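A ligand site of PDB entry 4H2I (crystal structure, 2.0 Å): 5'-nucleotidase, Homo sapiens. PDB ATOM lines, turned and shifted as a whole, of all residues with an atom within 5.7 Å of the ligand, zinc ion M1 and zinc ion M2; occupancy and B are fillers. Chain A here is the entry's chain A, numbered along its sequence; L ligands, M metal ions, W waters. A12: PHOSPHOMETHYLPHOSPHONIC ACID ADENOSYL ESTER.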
ATOM      1  N   ASP A  11      -8.760  -2.528 -16.357  1.00  0.00           N
ATOM      2  CA  ASP A  11      -8.234  -1.351 -17.128  1.00  0.00           C
ATOM      3  C   ASP A  11      -9.262  -0.709 -18.001  1.00  0.00           C
ATOM      4  O   ASP A  11      -8.988  -0.393 -19.165  1.00  0.00           O
ATOM      5  CB  ASP A  11      -6.950  -1.785 -17.932  1.00  0.00           C
ATOM      6  CG  ASP A  11      -5.895  -2.379 -17.016  1.00  0.00           C
ATOM      7  OD1 ASP A  11      -5.985  -3.624 -16.728  1.00  0.00           O
ATOM      8  OD2 ASP A  11      -4.954  -1.684 -16.594  1.00  0.00           O
ATOM      9  N   HIS A  13     -10.396   2.269 -17.514  1.00  0.00           N
ATOM     10  CA  HIS A  13      -9.789   3.597 -17.791  1.00  0.00           C
ATOM     11  C   HIS A  13     -10.833   4.601 -18.335  1.00  0.00           C
ATOM     12  O   HIS A  13     -10.714   5.182 -19.484  1.00  0.00           O
ATOM     13  CB  HIS A  13      -8.523   3.428 -18.730  1.00  0.00           C
ATOM     14  CG  HIS A  13      -7.338   2.905 -17.964  1.00  0.00           C
ATOM     15  ND1 HIS A  13      -6.896   3.528 -16.811  1.00  0.00           N
ATOM     16  CD2 HIS A  13      -6.624   1.755 -18.065  1.00  0.00           C
ATOM     17  CE1 HIS A  13      -5.906   2.830 -16.287  1.00  0.00           C
ATOM     18  NE2 HIS A  13      -5.715   1.745 -17.025  1.00  0.00           N
ATOM     19  N   ASP A  60      -7.786  -0.250 -12.153  1.00  0.00           N
ATOM     20  CA  ASP A  60      -7.506   0.732 -13.237  1.00  0.00           C
ATOM     21  C   ASP A  60      -8.818   1.129 -13.927  1.00  0.00           C
ATOM     22  O   ASP A  60      -8.848   1.263 -15.126  1.00  0.00           O
ATOM     23  CB  ASP A  60      -6.487   0.149 -14.250  1.00  0.00           C
ATOM     24  CG  ASP A  60      -5.005   0.479 -13.929  1.00  0.00           C
ATOM     25  OD1 ASP A  60      -4.764   0.948 -12.804  1.00  0.00           O
ATOM     26  OD2 ASP A  60      -4.082   0.245 -14.830  1.00  0.00           O
ATOM     27  N   GLY A  91      -6.216  -0.945  -8.404  1.00  0.00           N
ATOM     28  CA  GLY A  91      -5.078  -0.939  -9.347  1.00  0.00           C
ATOM     29  C   GLY A  91      -4.207   0.290  -9.083  1.00  0.00           C
ATOM     30  O   GLY A  91      -4.559   1.099  -8.255  1.00  0.00           O
ATOM     31  N   ASN A  92      -3.098   0.424  -9.788  1.00  0.00           N
ATOM     32  CA  ASN A  92      -2.204   1.545  -9.586  1.00  0.00           C
ATOM     33  C   ASN A  92      -2.874   2.869  -9.891  1.00  0.00           C
ATOM     34  O   ASN A  92      -2.672   3.830  -9.137  1.00  0.00           O
ATOM     35  CB  ASN A  92      -0.886   1.379 -10.398  1.00  0.00           C
ATOM     36  CG  ASN A  92      -1.132   1.029 -11.878  1.00  0.00           C
ATOM     37  OD1 ASN A  92      -1.704  -0.049 -12.235  1.00  0.00           O
ATOM     38  ND2 ASN A  92      -0.705   1.971 -12.792  1.00  0.00           N
ATOM     39  N   HIS A  93      -3.636   2.951 -10.993  1.00  0.00           N
ATOM     40  CA  HIS A  93      -4.293   4.242 -11.286  1.00  0.00           C
ATOM     41  C   HIS A  93      -5.325   4.737 -10.277  1.00  0.00           C
ATOM     42  O   HIS A  93      -5.643   5.952 -10.251  1.00  0.00           O
ATOM     43  CB  HIS A  93      -4.826   4.376 -12.730  1.00  0.00           C
ATOM     44  CG  HIS A  93      -3.734   4.364 -13.736  1.00  0.00           C
ATOM     45  ND1 HIS A  93      -2.991   5.486 -14.018  1.00  0.00           N
ATOM     46  CD2 HIS A  93      -3.141   3.339 -14.388  1.00  0.00           C
ATOM     47  CE1 HIS A  93      -2.013   5.170 -14.848  1.00  0.00           C
ATOM     48  NE2 HIS A  93      -2.067   3.876 -15.077  1.00  0.00           N
ATOM     49  N   ASP A  96      -3.812   7.740  -8.432  1.00  0.00           N
ATOM     50  CA  ASP A  96      -3.295   8.862  -9.219  1.00  0.00           C
ATOM     51  C   ASP A  96      -3.597  10.250  -8.597  1.00  0.00           C
ATOM     52  O   ASP A  96      -2.799  11.179  -8.752  1.00  0.00           O
ATOM     53  CB  ASP A  96      -3.853   8.787 -10.651  1.00  0.00           C
ATOM     54  CG  ASP A  96      -3.134   7.768 -11.509  1.00  0.00           C
ATOM     55  OD1 ASP A  96      -2.240   7.030 -11.017  1.00  0.00           O
ATOM     56  OD2 ASP A  96      -3.497   7.719 -12.684  1.00  0.00           O
ATOM     57  N   LEU A 159       4.581   4.335 -10.015  1.00  0.00           N
ATOM     58  CA  LEU A 159       3.592   4.602 -11.029  1.00  0.00           C
ATOM     59  C   LEU A 159       2.592   5.683 -10.679  1.00  0.00           C
ATOM     60  O   LEU A 159       2.083   6.338 -11.562  1.00  0.00           O
ATOM     61  CB  LEU A 159       2.838   3.308 -11.373  1.00  0.00           C
ATOM     62  CG  LEU A 159       3.646   2.266 -12.137  1.00  0.00           C
ATOM     63  CD1 LEU A 159       2.775   1.018 -12.208  1.00  0.00           C
ATOM     64  CD2 LEU A 159       4.026   2.788 -13.521  1.00  0.00           C
ATOM     65  N   HIS A 195      -4.220  -6.628  -9.559  1.00  0.00           N
ATOM     66  CA  HIS A 195      -3.803  -5.738 -10.628  1.00  0.00           C
ATOM     67  C   HIS A 195      -2.265  -5.630 -10.639  1.00  0.00           C
ATOM     68  O   HIS A 195      -1.684  -4.619 -10.170  1.00  0.00           O
ATOM     69  CB  HIS A 195      -4.406  -4.337 -10.322  1.00  0.00           C
ATOM     70  CG  HIS A 195      -4.256  -3.417 -11.460  1.00  0.00           C
ATOM     71  ND1 HIS A 195      -5.166  -3.379 -12.506  1.00  0.00           N
ATOM     72  CD2 HIS A 195      -3.235  -2.591 -11.811  1.00  0.00           C
ATOM     73  CE1 HIS A 195      -4.681  -2.589 -13.458  1.00  0.00           C
ATOM     74  NE2 HIS A 195      -3.552  -2.098 -13.040  1.00  0.00           N
ATOM     75  N   HIS A 218      -3.796  -4.924 -15.654  1.00  0.00           N
ATOM     76  CA  HIS A 218      -2.519  -4.127 -15.626  1.00  0.00           C
ATOM     77  C   HIS A 218      -1.716  -4.274 -16.905  1.00  0.00           C
ATOM     78  O   HIS A 218      -1.117  -3.295 -17.360  1.00  0.00           O
ATOM     79  CB  HIS A 218      -1.645  -4.392 -14.367  1.00  0.00           C
ATOM     80  CG  HIS A 218      -0.473  -3.435 -14.231  1.00  0.00           C
ATOM     81  ND1 HIS A 218      -0.654  -2.058 -14.159  1.00  0.00           N
ATOM     82  CD2 HIS A 218       0.860  -3.659 -14.132  1.00  0.00           C
ATOM     83  CE1 HIS A 218       0.541  -1.481 -14.063  1.00  0.00           C
ATOM     84  NE2 HIS A 218       1.483  -2.429 -14.092  1.00  0.00           N
ATOM     85  N   SER A 219      -1.670  -5.473 -17.484  1.00  0.00           N
ATOM     86  CA  SER A 219      -0.895  -5.646 -18.711  1.00  0.00           C
ATOM     87  C   SER A 219      -1.832  -5.657 -19.926  1.00  0.00           C
ATOM     88  O   SER A 219      -1.388  -5.792 -21.027  1.00  0.00           O
ATOM     89  CB  SER A 219      -0.038  -6.897 -18.622  1.00  0.00           C
ATOM     90  OG  SER A 219      -0.927  -7.967 -18.249  1.00  0.00           O
ATOM     91  N   ASN A 220      -3.130  -5.438 -19.747  1.00  0.00           N
ATOM     92  CA  ASN A 220      -4.133  -5.370 -20.835  1.00  0.00           C
ATOM     93  C   ASN A 220      -4.062  -6.633 -21.654  1.00  0.00           C
ATOM     94  O   ASN A 220      -4.197  -6.603 -22.875  1.00  0.00           O
ATOM     95  CB  ASN A 220      -3.926  -4.178 -21.760  1.00  0.00           C
ATOM     96  CG  ASN A 220      -3.732  -2.886 -20.988  1.00  0.00           C
ATOM     97  OD1 ASN A 220      -4.368  -2.602 -19.928  1.00  0.00           O
ATOM     98  ND2 ASN A 220      -2.723  -2.179 -21.411  1.00  0.00           N
ATOM     99  N   ARG A 329       4.179   1.653 -28.821  1.00  0.00           N
ATOM    100  CA  ARG A 329       5.144   0.866 -28.028  1.00  0.00           C
ATOM    101  C   ARG A 329       6.082   0.002 -28.858  1.00  0.00           C
ATOM    102  O   ARG A 329       6.878  -0.765 -28.315  1.00  0.00           O
ATOM    103  CB  ARG A 329       4.388   0.055 -26.990  1.00  0.00           C
ATOM    104  CG  ARG A 329       3.638   0.983 -26.047  1.00  0.00           C
ATOM    105  CD  ARG A 329       2.939   0.200 -24.906  1.00  0.00           C
ATOM    106  NE  ARG A 329       1.990   1.046 -24.176  1.00  0.00           N
ATOM    107  CZ  ARG A 329       1.550   0.819 -22.918  1.00  0.00           C
ATOM    108  NH1 ARG A 329       2.017  -0.223 -22.215  1.00  0.00           N
ATOM    109  NH2 ARG A 329       0.614   1.614 -22.373  1.00  0.00           N
ATOM    110  N   ASN A 365       7.999   8.691 -23.699  1.00  0.00           N
ATOM    111  CA  ASN A 365       7.567   7.328 -23.449  1.00  0.00           C
ATOM    112  C   ASN A 365       6.272   7.046 -24.208  1.00  0.00           C
ATOM    113  O   ASN A 365       5.197   7.725 -24.036  1.00  0.00           O
ATOM    114  CB  ASN A 365       7.447   7.043 -21.938  1.00  0.00           C
ATOM    115  CG  ASN A 365       6.499   8.002 -21.228  1.00  0.00           C
ATOM    116  OD1 ASN A 365       6.731   9.196 -21.238  1.00  0.00           O
ATOM    117  ND2 ASN A 365       5.472   7.453 -20.506  1.00  0.00           N
ATOM    118  N   GLY A 366       6.344   6.041 -25.046  1.00  0.00           N
ATOM    119  CA  GLY A 366       5.173   5.710 -25.881  1.00  0.00           C
ATOM    120  C   GLY A 366       3.973   5.283 -25.018  1.00  0.00           C
ATOM    121  O   GLY A 366       2.822   5.436 -25.443  1.00  0.00           O
ATOM    122  N   GLY A 367       4.215   4.785 -23.797  1.00  0.00           N
ATOM    123  CA  GLY A 367       3.115   4.307 -22.980  1.00  0.00           C
ATOM    124  C   GLY A 367       2.416   5.518 -22.352  1.00  0.00           C
ATOM    125  O   GLY A 367       1.343   5.361 -21.779  1.00  0.00           O
ATOM    126  N   GLY A 368       3.017   6.730 -22.443  1.00  0.00           N
ATOM    127  CA  GLY A 368       2.365   7.915 -21.905  1.00  0.00           C
ATOM    128  C   GLY A 368       1.301   8.436 -22.909  1.00  0.00           C
ATOM    129  O   GLY A 368       0.578   9.404 -22.626  1.00  0.00           O
ATOM    130  N   ARG A 370      -2.080   7.758 -24.584  1.00  0.00           N
ATOM    131  CA  ARG A 370      -3.084   6.793 -23.994  1.00  0.00           C
ATOM    132  C   ARG A 370      -4.325   6.617 -24.870  1.00  0.00           C
ATOM    133  O   ARG A 370      -5.204   5.820 -24.541  1.00  0.00           O
ATOM    134  CB  ARG A 370      -3.481   7.184 -22.529  1.00  0.00           C
ATOM    135  CG  ARG A 370      -2.295   7.440 -21.584  1.00  0.00           C
ATOM    136  CD  ARG A 370      -1.677   6.105 -21.163  1.00  0.00           C
ATOM    137  NE  ARG A 370      -2.638   5.367 -20.299  1.00  0.00           N
ATOM    138  CZ  ARG A 370      -2.304   4.328 -19.565  1.00  0.00           C
ATOM    139  NH1 ARG A 370      -3.202   3.733 -18.785  1.00  0.00           N
ATOM    140  NH2 ARG A 370      -1.021   3.928 -19.583  1.00  0.00           N
ATOM    141  N   PHE A 392      -2.729  12.465 -17.806  1.00  0.00           N
ATOM    142  CA  PHE A 392      -2.006  12.469 -16.524  1.00  0.00           C
ATOM    143  C   PHE A 392      -1.728  13.796 -15.860  1.00  0.00           C
ATOM    144  O   PHE A 392      -1.288  13.804 -14.691  1.00  0.00           O
ATOM    145  CB  PHE A 392      -0.695  11.682 -16.672  1.00  0.00           C
ATOM    146  CG  PHE A 392      -0.910  10.231 -17.071  1.00  0.00           C
ATOM    147  CD1 PHE A 392      -1.818   9.452 -16.360  1.00  0.00           C
ATOM    148  CD2 PHE A 392      -0.298   9.680 -18.180  1.00  0.00           C
ATOM    149  CE1 PHE A 392      -2.090   8.121 -16.737  1.00  0.00           C
ATOM    150  CE2 PHE A 392      -0.506   8.337 -18.524  1.00  0.00           C
ATOM    151  CZ  PHE A 392      -1.408   7.574 -17.809  1.00  0.00           C
ATOM    152  N   SER A 420       5.182  -4.918 -25.320  1.00  0.00           N
ATOM    153  CA  SER A 420       4.164  -3.812 -25.229  1.00  0.00           C
ATOM    154  C   SER A 420       4.361  -3.007 -23.937  1.00  0.00           C
ATOM    155  O   SER A 420       3.409  -2.628 -23.244  1.00  0.00           O
ATOM    156  CB  SER A 420       2.688  -4.297 -25.375  1.00  0.00           C
ATOM    157  OG  SER A 420       1.849  -3.207 -25.836  1.00  0.00           O
ATOM    158  N   THR A 421       5.602  -2.699 -23.664  1.00  0.00           N
ATOM    159  CA  THR A 421       5.919  -1.986 -22.446  1.00  0.00           C
ATOM    160  C   THR A 421       6.086  -0.523 -22.810  1.00  0.00           C
ATOM    161  O   THR A 421       6.458  -0.182 -23.975  1.00  0.00           O
ATOM    162  CB  THR A 421       7.216  -2.561 -21.771  1.00  0.00           C
ATOM    163  OG1 THR A 421       8.319  -2.565 -22.687  1.00  0.00           O
ATOM    164  CG2 THR A 421       7.000  -3.971 -21.235  1.00  0.00           C
ATOM    165  N   GLY A 422       5.905   0.356 -21.809  1.00  0.00           N
ATOM    166  CA  GLY A 422       5.698   1.785 -22.097  1.00  0.00           C
ATOM    167  C   GLY A 422       6.963   2.607 -22.357  1.00  0.00           C
ATOM    168  O   GLY A 422       6.878   3.765 -22.823  1.00  0.00           O
ATOM    169  N   GLU A 423       8.122   2.003 -22.080  1.00  0.00           N
ATOM    170  CA  GLU A 423       9.431   2.740 -22.159  1.00  0.00           C
ATOM    171  C   GLU A 423       9.913   3.044 -23.558  1.00  0.00           C
ATOM    172  O   GLU A 423      10.861   3.842 -23.710  1.00  0.00           O
ATOM    173  CB  GLU A 423      10.521   1.995 -21.392  1.00  0.00           C
ATOM    174  CG  GLU A 423      11.000   0.655 -22.003  1.00  0.00           C
ATOM    175  CD  GLU A 423      10.309  -0.597 -21.422  1.00  0.00           C
ATOM    176  OE1 GLU A 423      10.756  -1.718 -21.716  1.00  0.00           O
ATOM    177  OE2 GLU A 423       9.283  -0.492 -20.676  1.00  0.00           O
ATOM    178  N   PHE A 475       7.491  12.820 -15.959  1.00  0.00           N
ATOM    179  CA  PHE A 475       7.489  11.400 -15.687  1.00  0.00           C
ATOM    180  C   PHE A 475       8.868  10.794 -15.945  1.00  0.00           C
ATOM    181  O   PHE A 475       9.420  10.072 -15.112  1.00  0.00           O
ATOM    182  CB  PHE A 475       6.426  10.709 -16.527  1.00  0.00           C
ATOM    183  CG  PHE A 475       6.421   9.222 -16.386  1.00  0.00           C
ATOM    184  CD1 PHE A 475       5.929   8.594 -15.208  1.00  0.00           C
ATOM    185  CD2 PHE A 475       6.941   8.420 -17.399  1.00  0.00           C
ATOM    186  CE1 PHE A 475       5.892   7.200 -15.069  1.00  0.00           C
ATOM    187  CE2 PHE A 475       6.926   7.019 -17.261  1.00  0.00           C
ATOM    188  CZ  PHE A 475       6.364   6.410 -16.114  1.00  0.00           C
ATOM    189  N   ASP A 481       9.349   4.752 -15.740  1.00  0.00           N
ATOM    190  CA  ASP A 481       9.550   3.677 -16.741  1.00  0.00           C
ATOM    191  C   ASP A 481      10.956   3.102 -16.724  1.00  0.00           C
ATOM    192  O   ASP A 481      11.406   2.570 -17.722  1.00  0.00           O
ATOM    193  CB  ASP A 481       9.246   4.149 -18.212  1.00  0.00           C
ATOM    194  CG  ASP A 481       7.804   3.805 -18.685  1.00  0.00           C
ATOM    195  OD1 ASP A 481       7.124   2.970 -18.098  1.00  0.00           O
ATOM    196  OD2 ASP A 481       7.298   4.382 -19.651  1.00  0.00           O
HETATM  197  PB  A12 L   1      -1.383   1.008 -16.543  1.00  0.00           P
HETATM  198  O1B A12 L   1      -2.692   1.324 -17.051  1.00  0.00           O
HETATM  199  O2B A12 L   1      -0.601   2.427 -16.656  1.00  0.00           O
HETATM  200  O3B A12 L   1      -1.211   0.787 -15.033  1.00  0.00           O
HETATM  201  PA  A12 L   1      -0.165   0.057 -19.188  1.00  0.00           P
HETATM  202  O1A A12 L   1      -1.435   0.137 -19.900  1.00  0.00           O
HETATM  203  O2A A12 L   1       0.677  -1.130 -19.862  1.00  0.00           O
HETATM  204  C3A A12 L   1      -0.341  -0.260 -17.377  1.00  0.00           C
HETATM  205  O5' A12 L   1       0.531   1.471 -19.125  1.00  0.00           O
HETATM  206  C5' A12 L   1       1.869   1.530 -18.601  1.00  0.00           C
HETATM  207  C4' A12 L   1       2.693   2.647 -19.343  1.00  0.00           C
HETATM  208  O4' A12 L   1       1.941   3.863 -19.296  1.00  0.00           O
HETATM  209  C3' A12 L   1       3.896   3.036 -18.484  1.00  0.00           C
HETATM  210  O3' A12 L   1       4.873   2.094 -18.917  1.00  0.00           O
HETATM  211  C2' A12 L   1       4.208   4.509 -18.804  1.00  0.00           C
HETATM  212  O2' A12 L   1       4.907   4.492 -20.094  1.00  0.00           O
HETATM  213  C1' A12 L   1       2.771   4.978 -18.984  1.00  0.00           C
HETATM  214  N9  A12 L   1       2.369   5.615 -17.771  1.00  0.00           N
HETATM  215  C8  A12 L   1       1.729   5.076 -16.713  1.00  0.00           C
HETATM  216  N7  A12 L   1       1.539   6.012 -15.746  1.00  0.00           N
HETATM  217  C5  A12 L   1       2.066   7.173 -16.249  1.00  0.00           C
HETATM  218  C6  A12 L   1       2.256   8.536 -15.758  1.00  0.00           C
HETATM  219  N6  A12 L   1       1.758   8.852 -14.529  1.00  0.00           N
HETATM  220  N1  A12 L   1       2.881   9.437 -16.576  1.00  0.00           N
HETATM  221  C2  A12 L   1       3.281   9.123 -17.811  1.00  0.00           C
HETATM  222  N3  A12 L   1       3.224   7.890 -18.332  1.00  0.00           N
HETATM  223  C4  A12 L   1       2.614   6.906 -17.590  1.00  0.00           C
HETATM  224 ZN    ZN M   1      -4.418   0.212 -16.886  1.00  0.00          ZN
HETATM  225 ZN    ZN M   2      -2.275  -0.634 -13.935  1.00  0.00          ZN
HETATM  226  O   HOH W   1       3.192  -0.157 -16.008  1.00  0.00           O
HETATM  227  O   HOH W   2       1.788  -3.115 -17.502  1.00  0.00           O
HETATM  228  O   HOH W   3       2.911  12.092 -15.766  1.00  0.00           O
HETATM  229  O   HOH W   4       4.530  10.666 -20.195  1.00  0.00           O
HETATM  230  O   HOH W   5      -2.656   1.752 -21.904  1.00  0.00           O
HETATM  231  O   HOH W   6       1.605   2.218 -14.919  1.00  0.00           O
HETATM  232  O   HOH W   7       5.077  -0.638 -19.334  1.00  0.00           O
HETATM  233  O   HOH W   8      -4.231  -0.258 -18.732  1.00  0.00           O
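Water W8 lies within hydrogen-bond range of OD1 of Asn 220 (2.6 Å) and O1A of the ligand (3.1 Å). Water W7 bridges O3' of the ligand (2.8 Å) and N of Gly 422 (2.8 Å). Water W6 bridges O2B of the ligand and ND2 of Asn 92. Water W5 bridges an oxygen (O1A) of the ligand and the guanidinium group of Arg 329. Water W2 bridges the backbone carbonyl oxygen of His 218 and an oxygen (O2A) of the ligand.
NE2 of His 93 is in hydrogen-bond range of O2B of the ligand, at 2.6 Å. The side-chain amide nitrogen (ND2) of Asn 365 lies within hydrogen-bond range of an oxygen (O2') of the ligand, 3.0 Å away. O of Gly 422 lies within hydrogen-bond range of O2' of the ligand, at 3.4 Å. An oxygen (O2') of the ligand sits at hydrogen-bond distance from the side-chain carboxylate (OD2) of Asp 481. The side-chain amide nitrogen (ND2) of Asn 220 is in hydrogen-bond range of an oxygen (O1A) of the ligand, 3.1 Å away. An oxygen (O2A) of the ligand is in salt-bridge range of the guanidinium group (NH1) of Arg 329, 2.9 Å away. The guanidinium group of Arg 370 is in salt-bridge range of an oxygen (O2B) of the ligand (3.3 Å).
The nearest printed residue that does not touch zinc ion M2 is His 93 (4.1 Å).
Of the 25 residues printed, 3 come within 4 Å of zinc ion M1.
The backbone NH (N) of Gly 367 lies within hydrogen-bond range of the backbone carbonyl oxygen (O) of Gly 422 (3.0 Å). The side-chain carboxylate (OD2) of Asp 481 sits at hydrogen-bond distance from the backbone NH (N) of Glu 423 (3.5 Å). A ring nitrogen (ND1) of His 93 sits at hydrogen-bond distance from the side-chain carboxylate of Asp 96, at 2.6 Å. OD1 of Asp 11 is in hydrogen-bond range of N of His 218, 2.8 Å away. N of Gly 368 sits close to ND2 of Asn 365 (3.2 Å). The side-chain carboxylate (OD1) of Asp 60 lies within hydrogen-bond range of the backbone NH (N) of His 93. The backbone carbonyl oxygen (O) of Ser 420 lies within hydrogen-bond range of the guanidinium group (NH1) of Arg 329, 3.0 Å away. O of Gly 422 is in hydrogen-bond range of N of Gly 366, at 3.2 Å.
O4' of the ligand sits close to O of Gly 367, at 3.0 Å. Residues that only touch the ligand: Phe 475 (3.4 Å), Phe 392 (3.6 Å), Gly 368 (3.7 Å) and Leu 159 (3.9 Å). Hydrophobic or aromatic side chains within 4 Å of the ligand: His 13, His 93, His 218, Phe 392 and Phe 475. 17 residues have an atom within 4 Å of the ligand: Asp 11, His 13, Asp 60, Asn 92, His 93, Leu 159, His 218, Asn 220, Arg 329, Asn 365, Gly 367, Gly 368, Arg 370, Phe 392, Gly 422, Phe 475 and Asp 481. The nearest printed residue that does not touch the ligand is His 195 (4.2 Å).
Zinc ion M1 is bound by water W8 (1.9 Å), OD2 of Asp 11 (2.0 Å), NE2 of His 13 (2.0 Å), O1B of the ligand (2.1 Å) and OD2 of Asp 60 (2.1 Å).
Zinc ion M2 is bound by the side-chain amide oxygen (OD1) of Asn 92 (1.9 Å). Zinc ion M2 is bound by an oxygen (O3B) of the ligand. Zinc ion M2 is bound by NE2 of His 195. ND1 of His 218 binds zinc ion M2 (2.2 Å). Zinc ion M2 is bound by OD2 of Asp 60. Zinc ion M2 has five donor atoms within binding distance.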
